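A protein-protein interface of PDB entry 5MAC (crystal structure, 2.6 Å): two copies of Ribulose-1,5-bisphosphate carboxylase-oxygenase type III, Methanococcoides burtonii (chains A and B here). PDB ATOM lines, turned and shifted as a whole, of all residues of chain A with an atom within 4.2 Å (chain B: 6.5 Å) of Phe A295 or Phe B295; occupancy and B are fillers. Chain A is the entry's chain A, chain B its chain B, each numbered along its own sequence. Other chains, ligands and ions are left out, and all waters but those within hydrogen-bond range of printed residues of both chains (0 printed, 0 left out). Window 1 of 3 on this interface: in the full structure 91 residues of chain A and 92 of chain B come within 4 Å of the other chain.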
ATOM      1  N   LYS A 126     -28.769  -1.542 -11.848  1.00  0.00           N
ATOM      2  CA  LYS A 126     -29.965  -0.887 -11.334  1.00  0.00           C
ATOM      3  C   LYS A 126     -30.702  -1.826 -10.407  1.00  0.00           C
ATOM      4  O   LYS A 126     -31.234  -2.825 -10.877  1.00  0.00           O
ATOM      5  CB  LYS A 126     -30.883  -0.466 -12.502  1.00  0.00           C
ATOM      6  CG  LYS A 126     -31.836   0.673 -12.161  1.00  0.00           C
ATOM      7  CD  LYS A 126     -31.379   1.961 -12.816  1.00  0.00           C
ATOM      8  CE  LYS A 126     -32.374   3.082 -12.745  1.00  0.00           C
ATOM      9  NZ  LYS A 126     -31.699   4.391 -12.861  1.00  0.00           N
ATOM     10  N   ALA A 291     -33.629  15.257  -6.055  1.00  0.00           N
ATOM     11  CA  ALA A 291     -32.301  14.697  -6.424  1.00  0.00           C
ATOM     12  C   ALA A 291     -32.328  13.174  -6.702  1.00  0.00           C
ATOM     13  O   ALA A 291     -31.312  12.609  -7.099  1.00  0.00           O
ATOM     14  CB  ALA A 291     -31.224  15.038  -5.385  1.00  0.00           C
ATOM     15  N   HIS A 292     -33.495  12.519  -6.526  1.00  0.00           N
ATOM     16  CA  HIS A 292     -33.655  11.066  -6.729  1.00  0.00           C
ATOM     17  C   HIS A 292     -33.406  10.621  -8.190  1.00  0.00           C
ATOM     18  O   HIS A 292     -33.030   9.464  -8.418  1.00  0.00           O
ATOM     19  CB  HIS A 292     -35.051  10.602  -6.253  1.00  0.00           C
ATOM     20  CG  HIS A 292     -36.174  11.001  -7.166  1.00  0.00           C
ATOM     21  ND1 HIS A 292     -36.641  10.147  -8.134  1.00  0.00           N
ATOM     22  CD2 HIS A 292     -36.860  12.164  -7.251  1.00  0.00           C
ATOM     23  CE1 HIS A 292     -37.578  10.824  -8.785  1.00  0.00           C
ATOM     24  NE2 HIS A 292     -37.741  12.034  -8.281  1.00  0.00           N
ATOM     25  N   GLY A 293     -33.631  11.536  -9.143  1.00  0.00           N
ATOM     26  CA  GLY A 293     -33.451  11.300 -10.569  1.00  0.00           C
ATOM     27  C   GLY A 293     -32.113  10.714 -10.941  1.00  0.00           C
ATOM     28  O   GLY A 293     -32.031   9.942 -11.880  1.00  0.00           O
ATOM     29  N   ALA A 294     -31.045  11.065 -10.238  1.00  0.00           N
ATOM     30  CA  ALA A 294     -29.750  10.442 -10.515  1.00  0.00           C
ATOM     31  C   ALA A 294     -29.863   8.923 -10.430  1.00  0.00           C
ATOM     32  O   ALA A 294     -29.405   8.202 -11.327  1.00  0.00           O
ATOM     33  CB  ALA A 294     -28.734  10.920  -9.505  1.00  0.00           C
ATOM     34  N   PHE A 295     -30.532   8.442  -9.367  1.00  0.00           N
ATOM     35  CA  PHE A 295     -30.732   7.015  -9.127  1.00  0.00           C
ATOM     36  C   PHE A 295     -31.864   6.380  -9.887  1.00  0.00           C
ATOM     37  O   PHE A 295     -31.687   5.274 -10.361  1.00  0.00           O
ATOM     38  CB  PHE A 295     -31.021   6.767  -7.659  1.00  0.00           C
ATOM     39  CG  PHE A 295     -30.002   7.268  -6.680  1.00  0.00           C
ATOM     40  CD1 PHE A 295     -28.924   6.477  -6.316  1.00  0.00           C
ATOM     41  CD2 PHE A 295     -30.212   8.453  -5.985  1.00  0.00           C
ATOM     42  CE1 PHE A 295     -28.021   6.900  -5.341  1.00  0.00           C
ATOM     43  CE2 PHE A 295     -29.317   8.866  -5.001  1.00  0.00           C
ATOM     44  CZ  PHE A 295     -28.228   8.081  -4.682  1.00  0.00           C
ATOM     45  N   THR A 296     -33.052   6.996  -9.899  1.00  0.00           N
ATOM     46  CA  THR A 296     -34.274   6.367 -10.444  1.00  0.00           C
ATOM     47  C   THR A 296     -34.638   6.639 -11.887  1.00  0.00           C
ATOM     48  O   THR A 296     -35.536   5.988 -12.401  1.00  0.00           O
ATOM     49  CB  THR A 296     -35.490   6.752  -9.590  1.00  0.00           C
ATOM     50  OG1 THR A 296     -35.880   8.093  -9.878  1.00  0.00           O
ATOM     51  CG2 THR A 296     -35.267   6.548  -8.088  1.00  0.00           C
ATOM     52  N   ARG A 297     -33.958   7.539 -12.545  1.00  0.00           N
ATOM     53  CA  ARG A 297     -34.298   7.952 -13.906  1.00  0.00           C
ATOM     54  C   ARG A 297     -33.965   6.854 -14.934  1.00  0.00           C
ATOM     55  O   ARG A 297     -32.861   6.317 -14.915  1.00  0.00           O
ATOM     56  CB  ARG A 297     -33.611   9.304 -14.157  1.00  0.00           C
ATOM     57  CG  ARG A 297     -34.084  10.126 -15.279  1.00  0.00           C
ATOM     58  CD  ARG A 297     -35.498  10.635 -15.192  1.00  0.00           C
ATOM     59  NE  ARG A 297     -35.818  11.200 -16.505  1.00  0.00           N
ATOM     60  CZ  ARG A 297     -35.641  12.460 -16.882  1.00  0.00           C
ATOM     61  NH1 ARG A 297     -35.228  13.372 -16.014  1.00  0.00           N
ATOM     62  NH2 ARG A 297     -35.919  12.831 -18.124  1.00  0.00           N
ATOM     63  N   ILE A 302     -27.447   3.071 -14.174  1.00  0.00           N
ATOM     64  CA  ILE A 302     -26.918   2.803 -12.838  1.00  0.00           C
ATOM     65  C   ILE A 302     -27.770   3.531 -11.772  1.00  0.00           C
ATOM     66  O   ILE A 302     -28.024   4.731 -11.892  1.00  0.00           O
ATOM     67  CB  ILE A 302     -25.412   3.221 -12.765  1.00  0.00           C
ATOM     68  CG1 ILE A 302     -24.586   2.506 -13.877  1.00  0.00           C
ATOM     69  CG2 ILE A 302     -24.795   2.946 -11.367  1.00  0.00           C
ATOM     70  CD1 ILE A 302     -23.165   3.065 -14.051  1.00  0.00           C
ATOM     71  N   GLY A 303     -28.165   2.793 -10.727  1.00  0.00           N
ATOM     72  CA  GLY A 303     -28.930   3.333  -9.608  1.00  0.00           C
ATOM     73  C   GLY A 303     -29.931   2.378  -8.985  1.00  0.00           C
ATOM     74  O   GLY A 303     -29.576   1.278  -8.565  1.00  0.00           O
ATOM     75  N   PHE A 304     -31.171   2.824  -8.845  1.00  0.00           N
ATOM     76  CA  PHE A 304     -32.218   2.016  -8.241  1.00  0.00           C
ATOM     77  C   PHE A 304     -33.573   2.516  -8.674  1.00  0.00           C
ATOM     78  O   PHE A 304     -33.682   3.648  -9.086  1.00  0.00           O
ATOM     79  CB  PHE A 304     -32.103   1.996  -6.698  1.00  0.00           C
ATOM     80  CG  PHE A 304     -32.115   3.319  -5.951  1.00  0.00           C
ATOM     81  CD1 PHE A 304     -33.248   4.121  -5.943  1.00  0.00           C
ATOM     82  CD2 PHE A 304     -31.048   3.693  -5.147  1.00  0.00           C
ATOM     83  CE1 PHE A 304     -33.270   5.318  -5.249  1.00  0.00           C
ATOM     84  CE2 PHE A 304     -31.096   4.868  -4.407  1.00  0.00           C
ATOM     85  CZ  PHE A 304     -32.212   5.671  -4.462  1.00  0.00           C
ATOM     86  N   ILE B 113     -29.314  20.401  -8.130  1.00  0.00           N
ATOM     87  CA  ILE B 113     -29.307  18.980  -8.523  1.00  0.00           C
ATOM     88  C   ILE B 113     -30.512  18.263  -7.927  1.00  0.00           C
ATOM     89  O   ILE B 113     -30.464  17.060  -7.705  1.00  0.00           O
ATOM     90  CB  ILE B 113     -27.957  18.251  -8.248  1.00  0.00           C
ATOM     91  CG1 ILE B 113     -27.541  18.269  -6.745  1.00  0.00           C
ATOM     92  CG2 ILE B 113     -26.855  18.824  -9.133  1.00  0.00           C
ATOM     93  CD1 ILE B 113     -27.789  17.054  -6.006  1.00  0.00           C
ATOM     94  N   LEU B 117     -33.605  17.167 -12.095  1.00  0.00           N
ATOM     95  CA  LEU B 117     -33.101  15.873 -12.563  1.00  0.00           C
ATOM     96  C   LEU B 117     -34.209  14.916 -12.995  1.00  0.00           C
ATOM     97  O   LEU B 117     -33.910  13.951 -13.672  1.00  0.00           O
ATOM     98  CB  LEU B 117     -32.245  15.185 -11.469  1.00  0.00           C
ATOM     99  CG  LEU B 117     -30.950  15.861 -10.998  1.00  0.00           C
ATOM    100  CD1 LEU B 117     -30.054  14.867 -10.226  1.00  0.00           C
ATOM    101  CD2 LEU B 117     -30.152  16.428 -12.155  1.00  0.00           C
ATOM    102  N   LYS B 126     -26.483  16.861 -16.621  1.00  0.00           N
ATOM    103  CA  LYS B 126     -25.360  16.640 -15.699  1.00  0.00           C
ATOM    104  C   LYS B 126     -24.704  17.971 -15.297  1.00  0.00           C
ATOM    105  O   LYS B 126     -24.187  18.664 -16.154  1.00  0.00           O
ATOM    106  CB  LYS B 126     -24.307  15.713 -16.353  1.00  0.00           C
ATOM    107  CG  LYS B 126     -23.395  14.975 -15.354  1.00  0.00           C
ATOM    108  CD  LYS B 126     -23.438  13.489 -15.642  1.00  0.00           C
ATOM    109  CE  LYS B 126     -22.574  12.625 -14.765  1.00  0.00           C
ATOM    110  NZ  LYS B 126     -23.216  11.297 -14.578  1.00  0.00           N
ATOM    111  N   ILE B 266     -23.254  10.522   1.117  1.00  0.00           N
ATOM    112  CA  ILE B 266     -24.379  10.404   0.175  1.00  0.00           C
ATOM    113  C   ILE B 266     -25.612   9.751   0.869  1.00  0.00           C
ATOM    114  O   ILE B 266     -26.730  10.282   0.744  1.00  0.00           O
ATOM    115  CB  ILE B 266     -24.009   9.720  -1.204  1.00  0.00           C
ATOM    116  CG1 ILE B 266     -23.256  10.700  -2.173  1.00  0.00           C
ATOM    117  CG2 ILE B 266     -25.276   9.237  -1.930  1.00  0.00           C
ATOM    118  CD1 ILE B 266     -22.043  11.192  -1.759  1.00  0.00           C
ATOM    119  N   ALA B 291     -22.421   5.416  -3.147  1.00  0.00           N
ATOM    120  CA  ALA B 291     -23.683   5.649  -3.873  1.00  0.00           C
ATOM    121  C   ALA B 291     -23.656   6.888  -4.777  1.00  0.00           C
ATOM    122  O   ALA B 291     -24.659   7.203  -5.418  1.00  0.00           O
ATOM    123  CB  ALA B 291     -24.888   5.677  -2.933  1.00  0.00           C
ATOM    124  N   HIS B 292     -22.481   7.533  -4.891  1.00  0.00           N
ATOM    125  CA  HIS B 292     -22.264   8.694  -5.761  1.00  0.00           C
ATOM    126  C   HIS B 292     -22.317   8.307  -7.238  1.00  0.00           C
ATOM    127  O   HIS B 292     -22.546   9.171  -8.068  1.00  0.00           O
ATOM    128  CB  HIS B 292     -20.913   9.369  -5.444  1.00  0.00           C
ATOM    129  CG  HIS B 292     -19.739   8.642  -6.020  1.00  0.00           C
ATOM    130  ND1 HIS B 292     -19.146   9.057  -7.199  1.00  0.00           N
ATOM    131  CD2 HIS B 292     -19.163   7.483  -5.637  1.00  0.00           C
ATOM    132  CE1 HIS B 292     -18.210   8.166  -7.464  1.00  0.00           C
ATOM    133  NE2 HIS B 292     -18.196   7.193  -6.556  1.00  0.00           N
ATOM    134  N   GLY B 293     -22.053   7.038  -7.556  1.00  0.00           N
ATOM    135  CA  GLY B 293     -22.062   6.522  -8.920  1.00  0.00           C
ATOM    136  C   GLY B 293     -23.320   6.841  -9.708  1.00  0.00           C
ATOM    137  O   GLY B 293     -23.265   7.025 -10.926  1.00  0.00           O
ATOM    138  N   ALA B 294     -24.474   6.873  -9.037  1.00  0.00           N
ATOM    139  CA  ALA B 294     -25.721   7.234  -9.700  1.00  0.00           C
ATOM    140  C   ALA B 294     -25.610   8.645 -10.265  1.00  0.00           C
ATOM    141  O   ALA B 294     -26.043   8.900 -11.394  1.00  0.00           O
ATOM    142  CB  ALA B 294     -26.867   7.170  -8.723  1.00  0.00           C
ATOM    143  N   PHE B 295     -24.982   9.556  -9.493  1.00  0.00           N
ATOM    144  CA  PHE B 295     -24.780  10.944  -9.910  1.00  0.00           C
ATOM    145  C   PHE B 295     -23.645  11.165 -10.884  1.00  0.00           C
ATOM    146  O   PHE B 295     -23.818  11.893 -11.856  1.00  0.00           O
ATOM    147  CB  PHE B 295     -24.516  11.815  -8.685  1.00  0.00           C
ATOM    148  CG  PHE B 295     -25.695  11.946  -7.764  1.00  0.00           C
ATOM    149  CD1 PHE B 295     -26.711  12.854  -8.036  1.00  0.00           C
ATOM    150  CD2 PHE B 295     -25.740  11.248  -6.565  1.00  0.00           C
ATOM    151  CE1 PHE B 295     -27.785  13.007  -7.160  1.00  0.00           C
ATOM    152  CE2 PHE B 295     -26.810  11.401  -5.695  1.00  0.00           C
ATOM    153  CZ  PHE B 295     -27.839  12.268  -6.006  1.00  0.00           C
ATOM    154  N   THR B 296     -22.475  10.583 -10.588  1.00  0.00           N
ATOM    155  CA  THR B 296     -21.200  10.856 -11.256  1.00  0.00           C
ATOM    156  C   THR B 296     -20.746  10.014 -12.421  1.00  0.00           C
ATOM    157  O   THR B 296     -19.871  10.482 -13.158  1.00  0.00           O
ATOM    158  CB  THR B 296     -20.064  10.760 -10.235  1.00  0.00           C
ATOM    159  OG1 THR B 296     -19.831   9.390  -9.904  1.00  0.00           O
ATOM    160  CG2 THR B 296     -20.290  11.621  -9.007  1.00  0.00           C
ATOM    161  N   ARG B 297     -21.289   8.821 -12.630  1.00  0.00           N
ATOM    162  CA  ARG B 297     -20.747   7.976 -13.684  1.00  0.00           C
ATOM    163  C   ARG B 297     -21.087   8.394 -15.098  1.00  0.00           C
ATOM    164  O   ARG B 297     -22.185   8.859 -15.378  1.00  0.00           O
ATOM    165  CB  ARG B 297     -21.078   6.494 -13.459  1.00  0.00           C
ATOM    166  CG  ARG B 297     -19.955   5.912 -12.615  1.00  0.00           C
ATOM    167  CD  ARG B 297     -20.007   4.464 -12.451  1.00  0.00           C
ATOM    168  NE  ARG B 297     -19.657   3.699 -13.638  1.00  0.00           N
ATOM    169  CZ  ARG B 297     -19.558   2.374 -13.631  1.00  0.00           C
ATOM    170  NH1 ARG B 297     -19.765   1.693 -12.515  1.00  0.00           N
ATOM    171  NH2 ARG B 297     -19.266   1.716 -14.744  1.00  0.00           N
ATOM    172  N   ASN B 300     -24.301   7.563 -17.015  1.00  0.00           N
ATOM    173  CA  ASN B 300     -25.501   8.240 -16.540  1.00  0.00           C
ATOM    174  C   ASN B 300     -25.655   9.677 -17.038  1.00  0.00           C
ATOM    175  O   ASN B 300     -25.073  10.601 -16.451  1.00  0.00           O
ATOM    176  CB  ASN B 300     -25.534   8.224 -15.008  1.00  0.00           C
ATOM    177  CG  ASN B 300     -26.082   6.961 -14.379  1.00  0.00           C
ATOM    178  OD1 ASN B 300     -26.278   5.914 -15.004  1.00  0.00           O
ATOM    179  ND2 ASN B 300     -26.443   7.070 -13.138  1.00  0.00           N
ATOM    180  N   ILE B 302     -27.914  11.877 -16.443  1.00  0.00           N
ATOM    181  CA  ILE B 302     -28.495  12.709 -15.383  1.00  0.00           C
ATOM    182  C   ILE B 302     -27.622  12.621 -14.119  1.00  0.00           C
ATOM    183  O   ILE B 302     -27.249  11.528 -13.712  1.00  0.00           O
ATOM    184  CB  ILE B 302     -29.931  12.241 -15.052  1.00  0.00           C
ATOM    185  CG1 ILE B 302     -30.770  11.877 -16.324  1.00  0.00           C
ATOM    186  CG2 ILE B 302     -30.627  13.264 -14.165  1.00  0.00           C
ATOM    187  CD1 ILE B 302     -31.443  12.903 -16.943  1.00  0.00           C
ATOM    188  N   GLY B 303     -27.365  13.760 -13.481  1.00  0.00           N
ATOM    189  CA  GLY B 303     -26.579  13.790 -12.257  1.00  0.00           C
ATOM    190  C   GLY B 303     -25.646  14.970 -12.157  1.00  0.00           C
ATOM    191  O   GLY B 303     -26.019  16.084 -12.523  1.00  0.00           O
ATOM    192  N   PHE B 304     -24.445  14.732 -11.610  1.00  0.00           N
ATOM    193  CA  PHE B 304     -23.416  15.752 -11.400  1.00  0.00           C
ATOM    194  C   PHE B 304     -22.018  15.132 -11.453  1.00  0.00           C
ATOM    195  O   PHE B 304     -21.877  13.945 -11.185  1.00  0.00           O
ATOM    196  CB  PHE B 304     -23.624  16.499 -10.054  1.00  0.00           C
ATOM    197  CG  PHE B 304     -23.628  15.698  -8.765  1.00  0.00           C
ATOM    198  CD1 PHE B 304     -22.476  15.065  -8.310  1.00  0.00           C
ATOM    199  CD2 PHE B 304     -24.723  15.724  -7.918  1.00  0.00           C
ATOM    200  CE1 PHE B 304     -22.490  14.314  -7.140  1.00  0.00           C
ATOM    201  CE2 PHE B 304     -24.701  15.031  -6.706  1.00  0.00           C
ATOM    202  CZ  PHE B 304     -23.597  14.308  -6.342  1.00  0.00           C
ATOM    203  N   SER B 305     -20.991  15.947 -11.704  1.00  0.00           N
ATOM    204  CA  SER B 305     -19.610  15.487 -11.776  1.00  0.00           C
ATOM    205  C   SER B 305     -18.921  15.291 -10.423  1.00  0.00           C
ATOM    206  O   SER B 305     -19.290  15.923  -9.440  1.00  0.00           O
ATOM    207  CB  SER B 305     -18.787  16.483 -12.582  1.00  0.00           C
ATOM    208  OG  SER B 305     -18.546  17.664 -11.837  1.00  0.00           O
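The backbone carbonyl oxygen (O) of Phe A295 is in hydrogen-bond range of the side-chain amino group (NZ) of Lys A126 (2.7 Å).
The side-chain amino group of Lys A126 is in hydrogen-bond range of the backbone carbonyl oxygen of Arg A297, 3.0 Å away.
The side-chain amino group (NZ) of Lys B126 lies within hydrogen-bond range of the backbone carbonyl oxygen (O) of Phe B295.
NZ of Lys B126 sits at hydrogen-bond distance from O of Asn B300, 2.7 Å away.
The backbone carbonyl oxygen of Ala B294 sits at hydrogen-bond distance from the side-chain amide nitrogen of Asn B300.
The backbone NH (N) of Phe B304 is in hydrogen-bond range of the backbone carbonyl oxygen (O) of Phe B295.
Ala A294 touches its own counterpart, Ala B294.
Ala A294 touches Phe B295, and with the chains exchanged Phe A295 touches Ala B294.
Phe B295 touches its own counterpart, Phe A295.
Arg A297 touches Ile B302, and with the chains exchanged Ile A302 touches Arg B297.
Positions printed for both chains: 126, 291, 292, 293, 294, 295, 296, 297, 302, 303 and 304.
Hydrophobic or aromatic side chains of chain B that line the printed part of chain A: Leu B117, Ala B294, Phe B295 and Ile B302.
Of the 11 printed residues of chain A, 5 touch a printed residue of chain B.
Among the printed residues, no Asp or Glu carboxylate lies within 4 Å of a Lys or Arg side-chain nitrogen of the other chain.
O of Ile B113 touches CB of Ala A291 (3.2 Å).
Ala A291 touches Phe B295.
CD1 of Leu B117 touches N of Ala A294, at 3.9 Å.
Ala A294 touches Phe B295 (CB to CD1, 3.2 Å).
Asn B300 touches Ala A294.
Phe A295 touches Ala B291 (CE1 to O, 3.4 Å).
Ala B294 touches Phe A295.
Phe B295 touches Phe A295.
Arg A297 touches Ile B302.
Ile A302 touches Arg B297 (CD1 to NE, 3.6 Å).
The guanidinium group (NH1) of Arg A297 lies within hydrogen-bond range of the backbone carbonyl oxygen (O) of Leu B117.
ND2 of Asn B300 is in hydrogen-bond range of O of Ile A302.
The backbone carbonyl oxygen (O) of Ala A294 lies close to the backbone carbonyl oxygen (O) of Ala B294, 3.4 Å away.
Of the printed residues of chain B, Phe A295 touches Ala B291 (3.4 Å), Ala B294 (3.2 Å) and Phe B295 (3.6 Å).
Phe B295 touches just these residues of chain A: Ala A291, Ala A294 and Phe A295.
Of the printed residues of chain B, Ala A291 touches Ile B113 and Phe B295.
Printed residues of chain A within 4 Å of Ile B113: Ala A291.
Gly B293 touches none of the printed residues of chain A.
The nearest printed residue of chain A that does not touch Leu B117 is Ala A291 (4.1 Å).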
